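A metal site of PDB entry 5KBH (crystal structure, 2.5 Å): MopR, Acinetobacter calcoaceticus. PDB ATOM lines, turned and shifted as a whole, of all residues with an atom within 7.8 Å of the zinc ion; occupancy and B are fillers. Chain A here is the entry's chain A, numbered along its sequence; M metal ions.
SG of Cys 189 sits close to N of Val 182 (3.2 Å).
N of Trp 134 sits at hydrogen-bond distance from O of Cys 189 (2.9 Å).
The side-chain sulfur (SG) of Cys 181 lies close to the backbone NH (N) of Ala 154, 3.4 Å away.
The side-chain sulfur (SG) of Cys 181 sits close to the backbone NH (N) of Ala 183 (3.5 Å).
The side-chain sulfur of Cys 155 lies close to the backbone NH of Ala 140, at 3.7 Å.
The side-chain sulfur of Cys 155 lies close to the side-chain hydroxyl of Ser 137, 3.0 Å away.
The backbone NH of Ala 140 is in hydrogen-bond range of the side-chain hydroxyl of Ser 137 (3.1 Å).
Residues that only touch the zinc ion: Ala 140 (3.9 Å) and Val 182 (3.9 Å).
Along chain A the residues within 4 Å of the zinc ion span positions 140 to 189.
The zinc ion is bound by the side-chain sulfur (SG) of Cys 189 (2.2 Å), the side-chain carboxylate (OE2) of Glu 178 (2.2 Å), the side-chain sulfur (SG) of Cys 181 (2.3 Å) and the side-chain sulfur (SG) of Cys 155 (2.4 Å).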
ATOM      1  N   VAL A 112      16.437  -2.022   7.697  1.00  0.00           N
ATOM      2  CA  VAL A 112      15.249  -2.013   6.863  1.00  0.00           C
ATOM      3  C   VAL A 112      15.529  -2.773   5.588  1.00  0.00           C
ATOM      4  O   VAL A 112      16.668  -2.830   5.124  1.00  0.00           O
ATOM      5  CB  VAL A 112      14.738  -0.583   6.585  1.00  0.00           C
ATOM      6  CG1 VAL A 112      15.828   0.307   6.005  1.00  0.00           C
ATOM      7  CG2 VAL A 112      13.525  -0.593   5.670  1.00  0.00           C
ATOM      8  N   TRP A 134       9.868   0.411   2.319  1.00  0.00           N
ATOM      9  CA  TRP A 134      10.701   0.053   3.436  1.00  0.00           C
ATOM     10  C   TRP A 134       9.888  -0.992   4.188  1.00  0.00           C
ATOM     11  O   TRP A 134       8.797  -0.666   4.674  1.00  0.00           O
ATOM     12  CB  TRP A 134      10.978   1.278   4.321  1.00  0.00           C
ATOM     13  CG  TRP A 134      12.227   2.089   4.022  1.00  0.00           C
ATOM     14  CD1 TRP A 134      13.308   1.722   3.271  1.00  0.00           C
ATOM     15  CD2 TRP A 134      12.545   3.381   4.578  1.00  0.00           C
ATOM     16  NE1 TRP A 134      14.280   2.725   3.287  1.00  0.00           N
ATOM     17  CE2 TRP A 134      13.835   3.753   4.087  1.00  0.00           C
ATOM     18  CE3 TRP A 134      11.866   4.273   5.434  1.00  0.00           C
ATOM     19  CZ2 TRP A 134      14.438   4.979   4.415  1.00  0.00           C
ATOM     20  CZ3 TRP A 134      12.462   5.477   5.758  1.00  0.00           C
ATOM     21  CH2 TRP A 134      13.729   5.839   5.240  1.00  0.00           C
ATOM     22  N   SER A 137      11.006  -2.017   8.987  1.00  0.00           N
ATOM     23  CA  SER A 137      11.796  -0.959   9.577  1.00  0.00           C
ATOM     24  C   SER A 137      11.916  -1.190  11.076  1.00  0.00           C
ATOM     25  O   SER A 137      10.909  -1.316  11.756  1.00  0.00           O
ATOM     26  CB  SER A 137      11.157   0.406   9.329  1.00  0.00           C
ATOM     27  OG  SER A 137      11.535   1.321  10.343  1.00  0.00           O
ATOM     28  N   PHE A 138      13.139  -1.222  11.585  1.00  0.00           N
ATOM     29  CA  PHE A 138      13.350  -1.397  13.024  1.00  0.00           C
ATOM     30  C   PHE A 138      12.864  -0.151  13.780  1.00  0.00           C
ATOM     31  O   PHE A 138      12.405  -0.209  14.919  1.00  0.00           O
ATOM     32  CB  PHE A 138      14.818  -1.648  13.366  1.00  0.00           C
ATOM     33  CG  PHE A 138      15.593  -0.399  13.567  1.00  0.00           C
ATOM     34  CD1 PHE A 138      15.610   0.223  14.817  1.00  0.00           C
ATOM     35  CD2 PHE A 138      16.279   0.186  12.533  1.00  0.00           C
ATOM     36  CE1 PHE A 138      16.300   1.402  15.017  1.00  0.00           C
ATOM     37  CE2 PHE A 138      16.987   1.361  12.721  1.00  0.00           C
ATOM     38  CZ  PHE A 138      17.009   1.960  13.970  1.00  0.00           C
ATOM     39  N   GLU A 139      13.007   0.986  13.113  1.00  0.00           N
ATOM     40  CA  GLU A 139      12.803   2.273  13.741  1.00  0.00           C
ATOM     41  C   GLU A 139      11.341   2.484  14.076  1.00  0.00           C
ATOM     42  O   GLU A 139      10.990   2.978  15.156  1.00  0.00           O
ATOM     43  CB  GLU A 139      13.344   3.349  12.799  1.00  0.00           C
ATOM     44  CG  GLU A 139      13.537   4.671  13.489  1.00  0.00           C
ATOM     45  CD  GLU A 139      14.573   5.571  12.834  1.00  0.00           C
ATOM     46  OE1 GLU A 139      14.721   5.508  11.591  1.00  0.00           O
ATOM     47  OE2 GLU A 139      15.226   6.349  13.583  1.00  0.00           O
ATOM     48  N   ALA A 140      10.461   2.094  13.160  1.00  0.00           N
ATOM     49  CA  ALA A 140       9.037   2.128  13.381  1.00  0.00           C
ATOM     50  C   ALA A 140       8.642   1.232  14.547  1.00  0.00           C
ATOM     51  O   ALA A 140       7.826   1.606  15.383  1.00  0.00           O
ATOM     52  CB  ALA A 140       8.287   1.700  12.110  1.00  0.00           C
ATOM     53  N   GLU A 141       9.214   0.030  14.579  1.00  0.00           N
ATOM     54  CA  GLU A 141       8.955  -0.955  15.643  1.00  0.00           C
ATOM     55  C   GLU A 141       9.198  -0.334  17.012  1.00  0.00           C
ATOM     56  O   GLU A 141       8.327  -0.403  17.894  1.00  0.00           O
ATOM     57  CB  GLU A 141       9.876  -2.164  15.470  1.00  0.00           C
ATOM     58  CG  GLU A 141       9.244  -3.502  15.734  1.00  0.00           C
ATOM     59  CD  GLU A 141      10.187  -4.645  15.397  1.00  0.00           C
ATOM     60  OE1 GLU A 141      10.516  -4.807  14.197  1.00  0.00           O
ATOM     61  OE2 GLU A 141      10.607  -5.383  16.314  1.00  0.00           O
ATOM     62  N   GLN A 152       2.851  11.278  12.943  1.00  0.00           N
ATOM     63  CA  GLN A 152       3.823  11.627  11.899  1.00  0.00           C
ATOM     64  C   GLN A 152       4.751  10.427  11.611  1.00  0.00           C
ATOM     65  O   GLN A 152       4.834   9.508  12.429  1.00  0.00           O
ATOM     66  CB  GLN A 152       4.627  12.835  12.356  1.00  0.00           C
ATOM     67  CG  GLN A 152       5.562  12.528  13.518  1.00  0.00           C
ATOM     68  CD  GLN A 152       6.119  13.759  14.184  1.00  0.00           C
ATOM     69  OE1 GLN A 152       7.262  14.153  13.914  1.00  0.00           O
ATOM     70  NE2 GLN A 152       5.320  14.364  15.071  1.00  0.00           N
ATOM     71  N   PRO A 153       5.438  10.420  10.448  1.00  0.00           N
ATOM     72  CA  PRO A 153       6.371   9.338  10.169  1.00  0.00           C
ATOM     73  C   PRO A 153       7.495   9.292  11.194  1.00  0.00           C
ATOM     74  O   PRO A 153       7.931  10.336  11.680  1.00  0.00           O
ATOM     75  CB  PRO A 153       6.915   9.660   8.784  1.00  0.00           C
ATOM     76  CG  PRO A 153       6.524  11.040   8.507  1.00  0.00           C
ATOM     77  CD  PRO A 153       5.261  11.268   9.253  1.00  0.00           C
ATOM     78  N   ALA A 154       7.960   8.077  11.481  1.00  0.00           N
ATOM     79  CA  ALA A 154       8.833   7.803  12.635  1.00  0.00           C
ATOM     80  C   ALA A 154      10.253   7.372  12.294  1.00  0.00           C
ATOM     81  O   ALA A 154      11.097   7.278  13.202  1.00  0.00           O
ATOM     82  CB  ALA A 154       8.184   6.741  13.513  1.00  0.00           C
ATOM     83  N   CYS A 155      10.534   7.086  11.021  1.00  0.00           N
ATOM     84  CA  CYS A 155      11.822   6.512  10.616  1.00  0.00           C
ATOM     85  C   CYS A 155      12.912   7.572  10.288  1.00  0.00           C
ATOM     86  O   CYS A 155      13.477   7.626   9.192  1.00  0.00           O
ATOM     87  CB  CYS A 155      11.621   5.453   9.526  1.00  0.00           C
ATOM     88  SG  CYS A 155      10.516   4.117  10.113  1.00  0.00           S
ATOM     89  N   TRP A 156      13.265   8.307  11.330  1.00  0.00           N
ATOM     90  CA  TRP A 156      14.129   9.469  11.231  1.00  0.00           C
ATOM     91  C   TRP A 156      15.587   9.157  10.829  1.00  0.00           C
ATOM     92  O   TRP A 156      16.137   9.769   9.909  1.00  0.00           O
ATOM     93  CB  TRP A 156      14.130  10.242  12.557  1.00  0.00           C
ATOM     94  CG  TRP A 156      12.777  10.553  13.068  1.00  0.00           C
ATOM     95  CD1 TRP A 156      11.674  10.806  12.335  1.00  0.00           C
ATOM     96  CD2 TRP A 156      12.378  10.630  14.443  1.00  0.00           C
ATOM     97  NE1 TRP A 156      10.589  11.049  13.163  1.00  0.00           N
ATOM     98  CE2 TRP A 156      10.991  10.936  14.465  1.00  0.00           C
ATOM     99  CE3 TRP A 156      13.039  10.472  15.658  1.00  0.00           C
ATOM    100  CZ2 TRP A 156      10.280  11.089  15.644  1.00  0.00           C
ATOM    101  CZ3 TRP A 156      12.320  10.614  16.837  1.00  0.00           C
ATOM    102  CH2 TRP A 156      10.961  10.942  16.813  1.00  0.00           C
ATOM    103  N   LEU A 158      16.729   6.274   9.531  1.00  0.00           N
ATOM    104  CA  LEU A 158      16.698   5.661   8.192  1.00  0.00           C
ATOM    105  C   LEU A 158      16.619   6.700   7.093  1.00  0.00           C
ATOM    106  O   LEU A 158      17.308   6.583   6.071  1.00  0.00           O
ATOM    107  CB  LEU A 158      15.518   4.687   8.019  1.00  0.00           C
ATOM    108  CG  LEU A 158      15.403   3.504   8.979  1.00  0.00           C
ATOM    109  CD1 LEU A 158      14.325   2.529   8.511  1.00  0.00           C
ATOM    110  CD2 LEU A 158      16.710   2.784   9.172  1.00  0.00           C
ATOM    111  N   GLU A 178       9.148  10.540   3.880  1.00  0.00           N
ATOM    112  CA  GLU A 178       8.487   9.293   4.254  1.00  0.00           C
ATOM    113  C   GLU A 178       6.992   9.491   4.186  1.00  0.00           C
ATOM    114  O   GLU A 178       6.399  10.133   5.043  1.00  0.00           O
ATOM    115  CB  GLU A 178       8.935   8.787   5.623  1.00  0.00           C
ATOM    116  CG  GLU A 178       8.672   7.318   5.805  1.00  0.00           C
ATOM    117  CD  GLU A 178       8.932   6.780   7.220  1.00  0.00           C
ATOM    118  OE1 GLU A 178       9.314   7.527   8.146  1.00  0.00           O
ATOM    119  OE2 GLU A 178       8.734   5.568   7.382  1.00  0.00           O
ATOM    120  N   HIS A 180       4.444   7.201   3.892  1.00  0.00           N
ATOM    121  CA  HIS A 180       3.621   6.266   4.621  1.00  0.00           C
ATOM    122  C   HIS A 180       4.561   5.649   5.595  1.00  0.00           C
ATOM    123  O   HIS A 180       5.724   5.414   5.254  1.00  0.00           O
ATOM    124  CB  HIS A 180       3.063   5.186   3.704  1.00  0.00           C
ATOM    125  CG  HIS A 180       2.054   5.704   2.720  1.00  0.00           C
ATOM    126  ND1 HIS A 180       2.350   5.890   1.386  1.00  0.00           N
ATOM    127  CD2 HIS A 180       0.783   6.132   2.897  1.00  0.00           C
ATOM    128  CE1 HIS A 180       1.285   6.387   0.773  1.00  0.00           C
ATOM    129  NE2 HIS A 180       0.330   6.558   1.675  1.00  0.00           N
ATOM    130  N   CYS A 181       4.085   5.388   6.810  1.00  0.00           N
ATOM    131  CA  CYS A 181       4.919   4.838   7.843  1.00  0.00           C
ATOM    132  C   CYS A 181       4.162   3.825   8.699  1.00  0.00           C
ATOM    133  O   CYS A 181       3.065   4.093   9.164  1.00  0.00           O
ATOM    134  CB  CYS A 181       5.519   5.949   8.746  1.00  0.00           C
ATOM    135  SG  CYS A 181       6.737   5.306   9.947  1.00  0.00           S
ATOM    136  N   VAL A 182       4.776   2.676   8.931  1.00  0.00           N
ATOM    137  CA  VAL A 182       4.212   1.693   9.838  1.00  0.00           C
ATOM    138  C   VAL A 182       3.792   2.285  11.196  1.00  0.00           C
ATOM    139  O   VAL A 182       2.777   1.868  11.742  1.00  0.00           O
ATOM    140  CB  VAL A 182       5.166   0.494   9.978  1.00  0.00           C
ATOM    141  CG1 VAL A 182       4.876  -0.319  11.213  1.00  0.00           C
ATOM    142  CG2 VAL A 182       5.040  -0.396   8.746  1.00  0.00           C
ATOM    143  N   ALA A 183       4.504   3.276  11.732  1.00  0.00           N
ATOM    144  CA  ALA A 183       4.144   3.859  13.022  1.00  0.00           C
ATOM    145  C   ALA A 183       2.853   4.649  12.988  1.00  0.00           C
ATOM    146  O   ALA A 183       2.169   4.754  13.989  1.00  0.00           O
ATOM    147  CB  ALA A 183       5.265   4.727  13.556  1.00  0.00           C
ATOM    148  N   GLN A 184       2.516   5.204  11.835  1.00  0.00           N
ATOM    149  CA  GLN A 184       1.207   5.864  11.604  1.00  0.00           C
ATOM    150  C   GLN A 184       0.067   4.885  11.327  1.00  0.00           C
ATOM    151  O   GLN A 184      -1.057   5.297  11.198  1.00  0.00           O
ATOM    152  CB  GLN A 184       1.299   6.851  10.447  1.00  0.00           C
ATOM    153  CG  GLN A 184       2.262   7.988  10.743  1.00  0.00           C
ATOM    154  CD  GLN A 184       2.327   9.040   9.658  1.00  0.00           C
ATOM    155  OE1 GLN A 184       3.003   8.854   8.639  1.00  0.00           O
ATOM    156  NE2 GLN A 184       1.644  10.161   9.879  1.00  0.00           N
ATOM    157  N   HIS A 188       3.016  -0.747   5.138  1.00  0.00           N
ATOM    158  CA  HIS A 188       4.493  -0.686   5.051  1.00  0.00           C
ATOM    159  C   HIS A 188       4.906   0.787   5.089  1.00  0.00           C
ATOM    160  O   HIS A 188       4.048   1.662   5.038  1.00  0.00           O
ATOM    161  CB  HIS A 188       5.027  -1.407   3.791  1.00  0.00           C
ATOM    162  CG  HIS A 188       4.355  -0.985   2.507  1.00  0.00           C
ATOM    163  ND1 HIS A 188       4.734   0.132   1.790  1.00  0.00           N
ATOM    164  CD2 HIS A 188       3.338  -1.550   1.808  1.00  0.00           C
ATOM    165  CE1 HIS A 188       3.985   0.243   0.714  1.00  0.00           C
ATOM    166  NE2 HIS A 188       3.120  -0.758   0.705  1.00  0.00           N
ATOM    167  N   CYS A 189       6.207   1.062   5.210  1.00  0.00           N
ATOM    168  CA  CYS A 189       6.732   2.435   5.094  1.00  0.00           C
ATOM    169  C   CYS A 189       7.097   2.742   3.603  1.00  0.00           C
ATOM    170  O   CYS A 189       7.440   1.837   2.834  1.00  0.00           O
ATOM    171  CB  CYS A 189       7.970   2.643   5.990  1.00  0.00           C
ATOM    172  SG  CYS A 189       7.784   2.375   7.774  1.00  0.00           S
ATOM    173  N   ARG A 190       7.031   4.012   3.194  1.00  0.00           N
ATOM    174  CA  ARG A 190       7.379   4.376   1.815  1.00  0.00           C
ATOM    175  C   ARG A 190       8.097   5.710   1.734  1.00  0.00           C
ATOM    176  O   ARG A 190       7.694   6.671   2.376  1.00  0.00           O
ATOM    177  CB  ARG A 190       6.128   4.419   0.948  1.00  0.00           C
ATOM    178  CG  ARG A 190       6.348   4.984  -0.450  1.00  0.00           C
ATOM    179  CD  ARG A 190       5.267   4.510  -1.398  1.00  0.00           C
ATOM    180  NE  ARG A 190       5.166   5.365  -2.576  1.00  0.00           N
ATOM    181  CZ  ARG A 190       4.331   5.157  -3.594  1.00  0.00           C
ATOM    182  NH1 ARG A 190       3.487   4.107  -3.613  1.00  0.00           N
ATOM    183  NH2 ARG A 190       4.345   6.012  -4.618  1.00  0.00           N
ATOM    184  N   ILE A 191       9.142   5.762   0.908  1.00  0.00           N
ATOM    185  CA  ILE A 191       9.887   6.972   0.718  1.00  0.00           C
ATOM    186  C   ILE A 191       9.925   7.464  -0.733  1.00  0.00           C
ATOM    187  O   ILE A 191       9.818   6.679  -1.690  1.00  0.00           O
ATOM    188  CB  ILE A 191      11.319   6.863   1.272  1.00  0.00           C
ATOM    189  CG1 ILE A 191      12.134   5.768   0.583  1.00  0.00           C
ATOM    190  CG2 ILE A 191      11.301   6.617   2.766  1.00  0.00           C
ATOM    191  CD1 ILE A 191      13.615   5.819   0.920  1.00  0.00           C
HETATM  192 ZN    ZN M   1       8.434   4.081   9.018  1.00  0.00          ZN
